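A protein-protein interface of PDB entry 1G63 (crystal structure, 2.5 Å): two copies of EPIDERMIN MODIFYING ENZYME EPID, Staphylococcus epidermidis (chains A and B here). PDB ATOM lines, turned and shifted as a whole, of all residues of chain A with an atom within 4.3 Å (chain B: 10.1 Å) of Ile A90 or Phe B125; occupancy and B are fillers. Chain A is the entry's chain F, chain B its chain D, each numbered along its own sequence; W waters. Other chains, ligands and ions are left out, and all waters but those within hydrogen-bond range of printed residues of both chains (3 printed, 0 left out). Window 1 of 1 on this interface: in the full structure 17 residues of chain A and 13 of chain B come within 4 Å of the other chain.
ND2 of Asn A136 sits at hydrogen-bond distance from O of Leu A132. The backbone carbonyl oxygen (O) of Asn B88 lies close to the side-chain amide oxygen (OD1) of Asn B92, at 2.9 Å. O of Phe B125 sits close to OD1 of Asn B129, at 3.3 Å. The side-chain amide oxygen (OD1) of Asn B123 lies within hydrogen-bond range of the backbone NH (N) of Phe B125, 2.8 Å away. ND2 of Asn B88 is in hydrogen-bond range of OD1 of Asn B129 (3.1 Å). The backbone carbonyl oxygen of Ala B84 lies close to the side-chain amide oxygen of Asn B88 (3.3 Å).
Of the 14 printed residues of chain A, 8 touch a printed residue of chain B. Printed residues of chain A that touch a printed residue of chain B: Ile A90, Ala A91, Asn A92, Gly A93, Leu A132, Leu A133, Asn A136 and Val A138. Hydrophobic or aromatic side chains of chain A within 4 Å of the printed part of chain B: Leu A132, Leu A133 and Val A138. Along chain A the printed residues that touch a printed residue of chain B span positions 90 to 138. Of the 24 printed residues of chain B, 6 touch a printed residue of chain A. Hydrophobic or aromatic side chains of chain B within 4 Å of the printed part of chain A: Pro B124 and Phe B125. Among the printed residues, 12 pairs touch across the chains. Among the printed residues, no Asp or Glu carboxylate lies within 4 Å of a Lys or Arg side-chain nitrogen of the other chain.
Water W1 lies within hydrogen-bond range of the side-chain amide nitrogen (ND2) of Asn B92 (2.6 Å) and the side-chain amide nitrogen (ND2) of Asn A92 (3.0 Å). Water W3 lies within hydrogen-bond range of the side-chain amide nitrogen of Asn B129, the side-chain amide nitrogen of Asn A92 and the side-chain amide oxygen of Asn B92. Water W2 lies within hydrogen-bond range of O of Ile A90 and ND2 of Asn B123.
No residue of chain B comes within 4 Å of Thr A86. Ile A90 touches one residue of chain B. Of the printed residues of chain B, Asn A92 touches Asn B88, Asn B92 and Asn B129. Gly A93 touches two residues of chain B. Printed residues of chain B within 4 Å of Leu A132: Lys B128 (3.96 Å). Asn B85 touches none of the printed residues of chain A. Met B120 touches none of the printed residues of chain A. Of the printed residues of chain A, Pro B124 touches Asn A136. Printed residues of chain A within 4 Å of Phe B125: Ile A90, Ala A91, Gly A93, Leu A133, Asn A136 and Val A138. Of the printed residues of chain A, Lys B128 touches Leu A132. The nearest residue of chain B that does not touch Ile A90 is Asn B123 (5.6 Å). The nearest residue of chain A that does not touch Phe B125 is Leu A132 (4.1 Å). The nearest printed residue of chain A that does not touch Lys B128 is Asn A136 (4.02 Å).
Ile A90 touches Phe B125 (O to CD1, 3.6 Å). Ala A91 touches Phe B125 (O to CD2, 3.2 Å). CB of Asn B88 touches O of Asn A92, 3.5 Å away. N of Gly A93 touches CB of Phe B125, 3.9 Å away. Leu A132 touches Lys B128 (CD1 to NZ, 3.96 Å). Phe B125 touches Leu A133 (CZ to CD2, 3.5 Å). OD1 of Asn A136 touches CB of Pro B124, at 3.8 Å. CB of Asn A136 touches CE2 of Phe B125 (3.9 Å). Val A138 touches Phe B125 (CG2 to CZ, 3.9 Å).
Asn A92 touches Asn B88, but with the chains exchanged Asn A88 does not touch Asn B92 (7.3 Å). Asn A92 touches its own counterpart, Asn B92. Of the 12 pairs that touch across the chains among the printed residues, 1 has its exchanged pair printed and touching as well.
The side-chain amide oxygen (OD1) of Asn B129 lies close to the backbone carbonyl oxygen (O) of Asn A92 (3.1 Å). ND2 of Asn B92 sits close to ND2 of Asn A92. The side-chain amide oxygen (OD1) of Asn B88 lies close to the backbone carbonyl oxygen (O) of Gly A93, at 2.6 Å.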
ATOM      1  N   THR A  86      11.851  -8.630  11.442  1.00  0.00           N
ATOM      2  CA  THR A  86      10.667  -8.623  12.295  1.00  0.00           C
ATOM      3  C   THR A  86      11.031  -8.765  13.771  1.00  0.00           C
ATOM      4  O   THR A  86      10.423  -8.119  14.639  1.00  0.00           O
ATOM      5  CB  THR A  86       9.663  -9.730  11.875  1.00  0.00           C
ATOM      6  OG1 THR A  86       9.033  -9.343  10.646  1.00  0.00           O
ATOM      7  CG2 THR A  86       8.579  -9.935  12.953  1.00  0.00           C
ATOM      8  N   ILE A  87      12.027  -9.600  14.057  1.00  0.00           N
ATOM      9  CA  ILE A  87      12.472  -9.783  15.430  1.00  0.00           C
ATOM     10  C   ILE A  87      12.878  -8.409  15.983  1.00  0.00           C
ATOM     11  O   ILE A  87      12.421  -7.980  17.047  1.00  0.00           O
ATOM     12  CB  ILE A  87      13.680 -10.747  15.494  1.00  0.00           C
ATOM     13  CG1 ILE A  87      13.226 -12.181  15.191  1.00  0.00           C
ATOM     14  CG2 ILE A  87      14.342 -10.666  16.864  1.00  0.00           C
ATOM     15  CD1 ILE A  87      14.369 -13.163  15.028  1.00  0.00           C
ATOM     16  N   ASN A  88      13.718  -7.707  15.241  1.00  0.00           N
ATOM     17  CA  ASN A  88      14.183  -6.403  15.672  1.00  0.00           C
ATOM     18  C   ASN A  88      13.071  -5.362  15.769  1.00  0.00           C
ATOM     19  O   ASN A  88      13.124  -4.464  16.617  1.00  0.00           O
ATOM     20  CB  ASN A  88      15.301  -5.948  14.740  1.00  0.00           C
ATOM     21  CG  ASN A  88      16.536  -6.844  14.847  1.00  0.00           C
ATOM     22  OD1 ASN A  88      17.350  -6.929  13.924  1.00  0.00           O
ATOM     23  ND2 ASN A  88      16.678  -7.513  15.989  1.00  0.00           N
ATOM     24  N   LYS A  89      12.058  -5.475  14.914  1.00  0.00           N
ATOM     25  CA  LYS A  89      10.947  -4.534  14.965  1.00  0.00           C
ATOM     26  C   LYS A  89      10.143  -4.778  16.244  1.00  0.00           C
ATOM     27  O   LYS A  89       9.803  -3.840  16.983  1.00  0.00           O
ATOM     28  CB  LYS A  89      10.029  -4.709  13.751  1.00  0.00           C
ATOM     29  CG  LYS A  89      10.487  -4.019  12.482  1.00  0.00           C
ATOM     30  CD  LYS A  89       9.445  -4.237  11.394  1.00  0.00           C
ATOM     31  CE  LYS A  89       9.661  -3.358  10.178  1.00  0.00           C
ATOM     32  NZ  LYS A  89       8.564  -3.602   9.201  1.00  0.00           N
ATOM     33  N   ILE A  90       9.832  -6.043  16.496  1.00  0.00           N
ATOM     34  CA  ILE A  90       9.069  -6.400  17.684  1.00  0.00           C
ATOM     35  C   ILE A  90       9.807  -5.934  18.932  1.00  0.00           C
ATOM     36  O   ILE A  90       9.213  -5.362  19.836  1.00  0.00           O
ATOM     37  CB  ILE A  90       8.845  -7.920  17.765  1.00  0.00           C
ATOM     38  CG1 ILE A  90       8.005  -8.378  16.568  1.00  0.00           C
ATOM     39  CG2 ILE A  90       8.142  -8.279  19.072  1.00  0.00           C
ATOM     40  CD1 ILE A  90       7.800  -9.896  16.479  1.00  0.00           C
ATOM     41  N   ALA A  91      11.110  -6.174  18.972  1.00  0.00           N
ATOM     42  CA  ALA A  91      11.915  -5.775  20.110  1.00  0.00           C
ATOM     43  C   ALA A  91      11.828  -4.274  20.375  1.00  0.00           C
ATOM     44  O   ALA A  91      11.905  -3.838  21.536  1.00  0.00           O
ATOM     45  CB  ALA A  91      13.362  -6.179  19.886  1.00  0.00           C
ATOM     46  N   ASN A  92      11.674  -3.482  19.312  1.00  0.00           N
ATOM     47  CA  ASN A  92      11.602  -2.033  19.468  1.00  0.00           C
ATOM     48  C   ASN A  92      10.185  -1.484  19.438  1.00  0.00           C
ATOM     49  O   ASN A  92       9.993  -0.266  19.402  1.00  0.00           O
ATOM     50  CB  ASN A  92      12.429  -1.325  18.397  1.00  0.00           C
ATOM     51  CG  ASN A  92      13.922  -1.521  18.587  1.00  0.00           C
ATOM     52  OD1 ASN A  92      14.522  -2.403  17.967  1.00  0.00           O
ATOM     53  ND2 ASN A  92      14.535  -0.697  19.453  1.00  0.00           N
ATOM     54  N   GLY A  93       9.199  -2.377  19.447  1.00  0.00           N
ATOM     55  CA  GLY A  93       7.805  -1.952  19.434  1.00  0.00           C
ATOM     56  C   GLY A  93       7.307  -1.376  18.117  1.00  0.00           C
ATOM     57  O   GLY A  93       6.239  -0.758  18.047  1.00  0.00           O
ATOM     58  N   CYS A 103       1.802  -8.720  16.792  1.00  0.00           N
ATOM     59  CA  CYS A 103       2.847  -9.167  17.710  1.00  0.00           C
ATOM     60  C   CYS A 103       3.059  -8.218  18.892  1.00  0.00           C
ATOM     61  O   CYS A 103       3.434  -8.658  19.977  1.00  0.00           O
ATOM     62  CB  CYS A 103       4.163  -9.381  16.952  1.00  0.00           C
ATOM     63  SG  CYS A 103       4.125 -10.833  15.852  1.00  0.00           S
ATOM     64  N   LEU A 110       3.337 -14.676  22.614  1.00  0.00           N
ATOM     65  CA  LEU A 110       4.291 -14.770  21.516  1.00  0.00           C
ATOM     66  C   LEU A 110       5.433 -15.776  21.618  1.00  0.00           C
ATOM     67  O   LEU A 110       6.104 -15.872  22.642  1.00  0.00           O
ATOM     68  CB  LEU A 110       4.867 -13.374  21.259  1.00  0.00           C
ATOM     69  CG  LEU A 110       5.392 -13.029  19.865  1.00  0.00           C
ATOM     70  CD1 LEU A 110       4.290 -13.232  18.839  1.00  0.00           C
ATOM     71  CD2 LEU A 110       5.873 -11.589  19.858  1.00  0.00           C
ATOM     72  N   LEU A 132      16.761  -8.550  24.884  1.00  0.00           N
ATOM     73  CA  LEU A 132      15.699  -7.669  25.342  1.00  0.00           C
ATOM     74  C   LEU A 132      14.347  -8.379  25.339  1.00  0.00           C
ATOM     75  O   LEU A 132      13.566  -8.252  26.287  1.00  0.00           O
ATOM     76  CB  LEU A 132      15.638  -6.427  24.460  1.00  0.00           C
ATOM     77  CG  LEU A 132      14.684  -5.323  24.910  1.00  0.00           C
ATOM     78  CD1 LEU A 132      15.050  -4.872  26.312  1.00  0.00           C
ATOM     79  CD2 LEU A 132      14.769  -4.151  23.936  1.00  0.00           C
ATOM     80  N   LEU A 133      14.077  -9.136  24.277  1.00  0.00           N
ATOM     81  CA  LEU A 133      12.819  -9.863  24.156  1.00  0.00           C
ATOM     82  C   LEU A 133      12.679 -10.925  25.239  1.00  0.00           C
ATOM     83  O   LEU A 133      11.636 -11.042  25.881  1.00  0.00           O
ATOM     84  CB  LEU A 133      12.725 -10.520  22.772  1.00  0.00           C
ATOM     85  CG  LEU A 133      12.508  -9.593  21.571  1.00  0.00           C
ATOM     86  CD1 LEU A 133      12.757 -10.356  20.286  1.00  0.00           C
ATOM     87  CD2 LEU A 133      11.099  -9.026  21.607  1.00  0.00           C
ATOM     88  N   ASN A 136      11.905  -9.982  28.736  1.00  0.00           N
ATOM     89  CA  ASN A 136      10.600  -9.349  28.825  1.00  0.00           C
ATOM     90  C   ASN A 136       9.446 -10.301  28.551  1.00  0.00           C
ATOM     91  O   ASN A 136       8.378  -9.887  28.091  1.00  0.00           O
ATOM     92  CB  ASN A 136      10.532  -8.148  27.889  1.00  0.00           C
ATOM     93  CG  ASN A 136      11.189  -6.916  28.484  1.00  0.00           C
ATOM     94  OD1 ASN A 136      10.643  -6.283  29.390  1.00  0.00           O
ATOM     95  ND2 ASN A 136      12.375  -6.574  27.985  1.00  0.00           N
ATOM     96  N   VAL A 138       9.088 -12.746  26.307  1.00  0.00           N
ATOM     97  CA  VAL A 138       8.779 -13.155  24.950  1.00  0.00           C
ATOM     98  C   VAL A 138       9.630 -14.392  24.705  1.00  0.00           C
ATOM     99  O   VAL A 138      10.854 -14.347  24.814  1.00  0.00           O
ATOM    100  CB  VAL A 138       9.116 -12.048  23.932  1.00  0.00           C
ATOM    101  CG1 VAL A 138       8.910 -12.563  22.518  1.00  0.00           C
ATOM    102  CG2 VAL A 138       8.226 -10.841  24.179  1.00  0.00           C
ATOM    103  N   ALA B  84       0.928   3.591  18.639  1.00  0.00           N
ATOM    104  CA  ALA B  84       2.032   2.928  19.311  1.00  0.00           C
ATOM    105  C   ALA B  84       3.207   2.898  18.337  1.00  0.00           C
ATOM    106  O   ALA B  84       4.345   3.206  18.705  1.00  0.00           O
ATOM    107  CB  ALA B  84       1.629   1.506  19.707  1.00  0.00           C
ATOM    108  N   ASN B  85       2.914   2.551  17.086  1.00  0.00           N
ATOM    109  CA  ASN B  85       3.932   2.459  16.041  1.00  0.00           C
ATOM    110  C   ASN B  85       4.779   3.722  15.871  1.00  0.00           C
ATOM    111  O   ASN B  85       6.016   3.643  15.885  1.00  0.00           O
ATOM    112  CB  ASN B  85       3.286   2.091  14.694  1.00  0.00           C
ATOM    113  CG  ASN B  85       4.293   2.048  13.553  1.00  0.00           C
ATOM    114  OD1 ASN B  85       4.208   2.832  12.603  1.00  0.00           O
ATOM    115  ND2 ASN B  85       5.256   1.137  13.647  1.00  0.00           N
ATOM    116  N   ILE B  87       4.993   6.292  17.954  1.00  0.00           N
ATOM    117  CA  ILE B  87       5.634   6.608  19.225  1.00  0.00           C
ATOM    118  C   ILE B  87       6.953   5.855  19.288  1.00  0.00           C
ATOM    119  O   ILE B  87       7.999   6.445  19.555  1.00  0.00           O
ATOM    120  CB  ILE B  87       4.748   6.182  20.426  1.00  0.00           C
ATOM    121  CG1 ILE B  87       3.540   7.117  20.543  1.00  0.00           C
ATOM    122  CG2 ILE B  87       5.559   6.199  21.715  1.00  0.00           C
ATOM    123  CD1 ILE B  87       2.509   6.648  21.568  1.00  0.00           C
ATOM    124  N   ASN B  88       6.899   4.554  19.012  1.00  0.00           N
ATOM    125  CA  ASN B  88       8.092   3.715  19.045  1.00  0.00           C
ATOM    126  C   ASN B  88       9.130   4.086  17.976  1.00  0.00           C
ATOM    127  O   ASN B  88      10.333   3.968  18.204  1.00  0.00           O
ATOM    128  CB  ASN B  88       7.677   2.249  18.940  1.00  0.00           C
ATOM    129  CG  ASN B  88       6.897   1.784  20.168  1.00  0.00           C
ATOM    130  OD1 ASN B  88       6.140   0.812  20.116  1.00  0.00           O
ATOM    131  ND2 ASN B  88       7.089   2.479  21.287  1.00  0.00           N
ATOM    132  N   LYS B  89       8.677   4.552  16.816  1.00  0.00           N
ATOM    133  CA  LYS B  89       9.608   4.957  15.764  1.00  0.00           C
ATOM    134  C   LYS B  89      10.344   6.222  16.202  1.00  0.00           C
ATOM    135  O   LYS B  89      11.570   6.319  16.077  1.00  0.00           O
ATOM    136  CB  LYS B  89       8.864   5.251  14.461  1.00  0.00           C
ATOM    137  CG  LYS B  89       8.453   4.036  13.649  1.00  0.00           C
ATOM    138  CD  LYS B  89       7.806   4.509  12.358  1.00  0.00           C
ATOM    139  CE  LYS B  89       7.685   3.405  11.331  1.00  0.00           C
ATOM    140  NZ  LYS B  89       7.056   3.957  10.096  1.00  0.00           N
ATOM    141  N   ALA B  91      10.840   7.318  19.208  1.00  0.00           N
ATOM    142  CA  ALA B  91      11.726   6.970  20.306  1.00  0.00           C
ATOM    143  C   ALA B  91      13.046   6.387  19.811  1.00  0.00           C
ATOM    144  O   ALA B  91      14.091   6.581  20.445  1.00  0.00           O
ATOM    145  CB  ALA B  91      11.035   5.978  21.241  1.00  0.00           C
ATOM    146  N   ASN B  92      13.009   5.675  18.684  1.00  0.00           N
ATOM    147  CA  ASN B  92      14.226   5.078  18.134  1.00  0.00           C
ATOM    148  C   ASN B  92      14.845   5.890  16.993  1.00  0.00           C
ATOM    149  O   ASN B  92      15.781   5.433  16.330  1.00  0.00           O
ATOM    150  CB  ASN B  92      13.963   3.648  17.647  1.00  0.00           C
ATOM    151  CG  ASN B  92      13.709   2.674  18.783  1.00  0.00           C
ATOM    152  OD1 ASN B  92      12.561   2.398  19.146  1.00  0.00           O
ATOM    153  ND2 ASN B  92      14.782   2.143  19.350  1.00  0.00           N
ATOM    154  N   ILE B  94      13.599   6.568  14.150  1.00  0.00           N
ATOM    155  CA  ILE B  94      13.234   6.085  12.825  1.00  0.00           C
ATOM    156  C   ILE B  94      12.325   7.090  12.144  1.00  0.00           C
ATOM    157  O   ILE B  94      11.260   7.425  12.649  1.00  0.00           O
ATOM    158  CB  ILE B  94      12.543   4.727  12.922  1.00  0.00           C
ATOM    159  CG1 ILE B  94      13.553   3.716  13.454  1.00  0.00           C
ATOM    160  CG2 ILE B  94      11.995   4.296  11.560  1.00  0.00           C
ATOM    161  CD1 ILE B  94      12.958   2.404  13.711  1.00  0.00           C
ATOM    162  N   MET B 116      -4.654   4.199  21.723  1.00  0.00           N
ATOM    163  CA  MET B 116      -4.624   2.805  21.313  1.00  0.00           C
ATOM    164  C   MET B 116      -5.445   1.998  22.303  1.00  0.00           C
ATOM    165  O   MET B 116      -5.836   2.499  23.354  1.00  0.00           O
ATOM    166  CB  MET B 116      -3.184   2.293  21.330  1.00  0.00           C
ATOM    167  CG  MET B 116      -2.547   2.373  22.706  1.00  0.00           C
ATOM    168  SD  MET B 116      -0.791   2.051  22.742  1.00  0.00           S
ATOM    169  CE  MET B 116      -0.122   3.681  22.285  1.00  0.00           C
ATOM    170  N   ARG B 119      -4.790  -2.916  25.801  1.00  0.00           N
ATOM    171  CA  ARG B 119      -3.829  -4.013  25.751  1.00  0.00           C
ATOM    172  C   ARG B 119      -2.521  -3.633  25.063  1.00  0.00           C
ATOM    173  O   ARG B 119      -1.459  -4.106  25.459  1.00  0.00           O
ATOM    174  CB  ARG B 119      -4.435  -5.238  25.061  1.00  0.00           C
ATOM    175  CG  ARG B 119      -3.414  -6.350  24.853  1.00  0.00           C
ATOM    176  CD  ARG B 119      -4.071  -7.689  24.599  1.00  0.00           C
ATOM    177  NE  ARG B 119      -4.762  -8.180  25.774  1.00  0.00           N
ATOM    178  CZ  ARG B 119      -5.693  -9.128  25.789  1.00  0.00           C
ATOM    179  NH1 ARG B 119      -6.227  -9.470  26.952  1.00  0.00           N
ATOM    180  NH2 ARG B 119      -6.102  -9.721  24.669  1.00  0.00           N
ATOM    181  N   MET B 120      -2.596  -2.790  24.036  1.00  0.00           N
ATOM    182  CA  MET B 120      -1.393  -2.360  23.323  1.00  0.00           C
ATOM    183  C   MET B 120      -0.580  -1.463  24.239  1.00  0.00           C
ATOM    184  O   MET B 120       0.655  -1.482  24.223  1.00  0.00           O
ATOM    185  CB  MET B 120      -1.756  -1.578  22.060  1.00  0.00           C
ATOM    186  CG  MET B 120      -2.476  -2.375  20.993  1.00  0.00           C
ATOM    187  SD  MET B 120      -2.945  -1.293  19.624  1.00  0.00           S
ATOM    188  CE  MET B 120      -1.332  -1.020  18.841  1.00  0.00           C
ATOM    189  N   TRP B 121      -1.293  -0.680  25.043  1.00  0.00           N
ATOM    190  CA  TRP B 121      -0.685   0.252  25.985  1.00  0.00           C
ATOM    191  C   TRP B 121       0.198  -0.461  27.015  1.00  0.00           C
ATOM    192  O   TRP B 121       1.161   0.121  27.539  1.00  0.00           O
ATOM    193  CB  TRP B 121      -1.789   1.047  26.691  1.00  0.00           C
ATOM    194  CG  TRP B 121      -1.289   2.080  27.652  1.00  0.00           C
ATOM    195  CD1 TRP B 121      -1.470   2.092  29.008  1.00  0.00           C
ATOM    196  CD2 TRP B 121      -0.525   3.252  27.337  1.00  0.00           C
ATOM    197  NE1 TRP B 121      -0.867   3.200  29.556  1.00  0.00           N
ATOM    198  CE2 TRP B 121      -0.279   3.929  28.553  1.00  0.00           C
ATOM    199  CE3 TRP B 121      -0.027   3.798  26.148  1.00  0.00           C
ATOM    200  CZ2 TRP B 121       0.449   5.129  28.613  1.00  0.00           C
ATOM    201  CZ3 TRP B 121       0.698   4.994  26.208  1.00  0.00           C
ATOM    202  CH2 TRP B 121       0.926   5.642  27.434  1.00  0.00           C
ATOM    203  N   GLY B 122      -0.124  -1.721  27.300  1.00  0.00           N
ATOM    204  CA  GLY B 122       0.658  -2.470  28.269  1.00  0.00           C
ATOM    205  C   GLY B 122       1.946  -3.084  27.737  1.00  0.00           C
ATOM    206  O   GLY B 122       2.682  -3.727  28.494  1.00  0.00           O
ATOM    207  N   ASN B 123       2.233  -2.892  26.449  1.00  0.00           N
ATOM    208  CA  ASN B 123       3.438  -3.464  25.855  1.00  0.00           C
ATOM    209  C   ASN B 123       4.707  -2.906  26.504  1.00  0.00           C
ATOM    210  O   ASN B 123       4.902  -1.686  26.588  1.00  0.00           O
ATOM    211  CB  ASN B 123       3.448  -3.218  24.343  1.00  0.00           C
ATOM    212  CG  ASN B 123       4.626  -3.884  23.652  1.00  0.00           C
ATOM    213  OD1 ASN B 123       5.758  -3.400  23.717  1.00  0.00           O
ATOM    214  ND2 ASN B 123       4.362  -5.007  22.991  1.00  0.00           N
ATOM    215  N   PRO B 124       5.595  -3.804  26.968  1.00  0.00           N
ATOM    216  CA  PRO B 124       6.865  -3.470  27.627  1.00  0.00           C
ATOM    217  C   PRO B 124       7.767  -2.583  26.786  1.00  0.00           C
ATOM    218  O   PRO B 124       8.366  -1.629  27.284  1.00  0.00           O
ATOM    219  CB  PRO B 124       7.509  -4.839  27.872  1.00  0.00           C
ATOM    220  CG  PRO B 124       6.340  -5.790  27.893  1.00  0.00           C
ATOM    221  CD  PRO B 124       5.472  -5.261  26.785  1.00  0.00           C
ATOM    222  N   PHE B 125       7.870  -2.914  25.504  1.00  0.00           N
ATOM    223  CA  PHE B 125       8.730  -2.169  24.587  1.00  0.00           C
ATOM    224  C   PHE B 125       8.187  -0.768  24.330  1.00  0.00           C
ATOM    225  O   PHE B 125       8.956   0.188  24.218  1.00  0.00           O
ATOM    226  CB  PHE B 125       8.884  -2.975  23.295  1.00  0.00           C
ATOM    227  CG  PHE B 125       9.104  -4.444  23.543  1.00  0.00           C
ATOM    228  CD1 PHE B 125       8.111  -5.371  23.239  1.00  0.00           C
ATOM    229  CD2 PHE B 125      10.280  -4.893  24.140  1.00  0.00           C
ATOM    230  CE1 PHE B 125       8.282  -6.740  23.527  1.00  0.00           C
ATOM    231  CE2 PHE B 125      10.469  -6.250  24.436  1.00  0.00           C
ATOM    232  CZ  PHE B 125       9.464  -7.181  24.129  1.00  0.00           C
ATOM    233  N   LEU B 126       6.866  -0.640  24.254  1.00  0.00           N
ATOM    234  CA  LEU B 126       6.255   0.666  24.048  1.00  0.00           C
ATOM    235  C   LEU B 126       6.560   1.533  25.267  1.00  0.00           C
ATOM    236  O   LEU B 126       7.072   2.646  25.136  1.00  0.00           O
ATOM    237  CB  LEU B 126       4.734   0.539  23.896  1.00  0.00           C
ATOM    238  CG  LEU B 126       3.929   1.844  24.039  1.00  0.00           C
ATOM    239  CD1 LEU B 126       4.284   2.823  22.931  1.00  0.00           C
ATOM    240  CD2 LEU B 126       2.441   1.522  24.007  1.00  0.00           C
ATOM    241  N   GLN B 127       6.238   1.007  26.451  1.00  0.00           N
ATOM    242  CA  GLN B 127       6.462   1.719  27.712  1.00  0.00           C
ATOM    243  C   GLN B 127       7.914   2.130  27.915  1.00  0.00           C
ATOM    244  O   GLN B 127       8.199   3.241  28.373  1.00  0.00           O
ATOM    245  CB  GLN B 127       5.986   0.863  28.891  1.00  0.00           C
ATOM    246  CG  GLN B 127       4.475   0.789  29.010  1.00  0.00           C
ATOM    247  CD  GLN B 127       3.839   2.166  28.890  1.00  0.00           C
ATOM    248  OE1 GLN B 127       4.328   3.140  29.478  1.00  0.00           O
ATOM    249  NE2 GLN B 127       2.744   2.259  28.127  1.00  0.00           N
ATOM    250  N   LYS B 128       8.833   1.234  27.574  1.00  0.00           N
ATOM    251  CA  LYS B 128      10.252   1.530  27.708  1.00  0.00           C
ATOM    252  C   LYS B 128      10.601   2.728  26.816  1.00  0.00           C
ATOM    253  O   LYS B 128      11.399   3.586  27.191  1.00  0.00           O
ATOM    254  CB  LYS B 128      11.060   0.295  27.319  1.00  0.00           C
ATOM    255  CG  LYS B 128      12.550   0.415  27.543  1.00  0.00           C
ATOM    256  CD  LYS B 128      13.184  -0.967  27.734  1.00  0.00           C
ATOM    257  CE  LYS B 128      12.688  -1.634  29.025  1.00  0.00           C
ATOM    258  NZ  LYS B 128      13.394  -2.919  29.327  1.00  0.00           N
ATOM    259  N   ASN B 129       9.979   2.790  25.640  1.00  0.00           N
ATOM    260  CA  ASN B 129      10.217   3.888  24.699  1.00  0.00           C
ATOM    261  C   ASN B 129       9.580   5.181  25.188  1.00  0.00           C
ATOM    262  O   ASN B 129      10.112   6.267  24.960  1.00  0.00           O
ATOM    263  CB  ASN B 129       9.661   3.535  23.313  1.00  0.00           C
ATOM    264  CG  ASN B 129      10.540   2.548  22.559  1.00  0.00           C
ATOM    265  OD1 ASN B 129      10.082   1.881  21.628  1.00  0.00           O
ATOM    266  ND2 ASN B 129      11.811   2.460  22.946  1.00  0.00           N
ATOM    267  N   ILE B 130       8.438   5.064  25.852  1.00  0.00           N
ATOM    268  CA  ILE B 130       7.758   6.244  26.371  1.00  0.00           C
ATOM    269  C   ILE B 130       8.612   6.892  27.461  1.00  0.00           C
ATOM    270  O   ILE B 130       8.689   8.119  27.554  1.00  0.00           O
ATOM    271  CB  ILE B 130       6.369   5.881  26.936  1.00  0.00           C
ATOM    272  CG1 ILE B 130       5.400   5.638  25.773  1.00  0.00           C
ATOM    273  CG2 ILE B 130       5.851   7.003  27.854  1.00  0.00           C
ATOM    274  CD1 ILE B 130       3.980   5.317  26.205  1.00  0.00           C
ATOM    275  N   ASP B 131       9.249   6.063  28.283  1.00  0.00           N
ATOM    276  CA  ASP B 131      10.124   6.559  29.339  1.00  0.00           C
ATOM    277  C   ASP B 131      11.294   7.254  28.654  1.00  0.00           C
ATOM    278  O   ASP B 131      11.689   8.358  29.034  1.00  0.00           O
ATOM    279  CB  ASP B 131      10.650   5.404  30.197  1.00  0.00           C
ATOM    280  CG  ASP B 131       9.568   4.775  31.068  1.00  0.00           C
ATOM    281  OD1 ASP B 131       9.773   3.630  31.537  1.00  0.00           O
ATOM    282  OD2 ASP B 131       8.521   5.427  31.292  1.00  0.00           O
ATOM    283  N   LEU B 132      11.835   6.611  27.626  1.00  0.00           N
ATOM    284  CA  LEU B 132      12.962   7.169  26.900  1.00  0.00           C
ATOM    285  C   LEU B 132      12.631   8.548  26.346  1.00  0.00           C
ATOM    286  O   LEU B 132      13.444   9.466  26.415  1.00  0.00           O
ATOM    287  CB  LEU B 132      13.360   6.235  25.763  1.00  0.00           C
ATOM    288  CG  LEU B 132      14.646   6.594  25.017  1.00  0.00           C
ATOM    289  CD1 LEU B 132      15.818   6.669  25.994  1.00  0.00           C
ATOM    290  CD2 LEU B 132      14.913   5.540  23.956  1.00  0.00           C
ATOM    291  N   LEU B 133      11.432   8.692  25.795  1.00  0.00           N
ATOM    292  CA  LEU B 133      11.002   9.963  25.229  1.00  0.00           C
ATOM    293  C   LEU B 133      10.896  11.040  26.294  1.00  0.00           C
ATOM    294  O   LEU B 133      11.367  12.165  26.101  1.00  0.00           O
ATOM    295  CB  LEU B 133       9.647   9.801  24.536  1.00  0.00           C
ATOM    296  CG  LEU B 133       9.630   9.009  23.224  1.00  0.00           C
ATOM    297  CD1 LEU B 133       8.202   8.682  22.849  1.00  0.00           C
ATOM    298  CD2 LEU B 133      10.306   9.819  22.115  1.00  0.00           C
HETATM  299  O   HOH W   1      16.489   0.990  21.016  1.00  0.00           O
HETATM  300  O   HOH W   2       6.221  -5.210  20.179  1.00  0.00           O
HETATM  301  O   HOH W   3      12.887   0.522  21.401  1.00  0.00           O
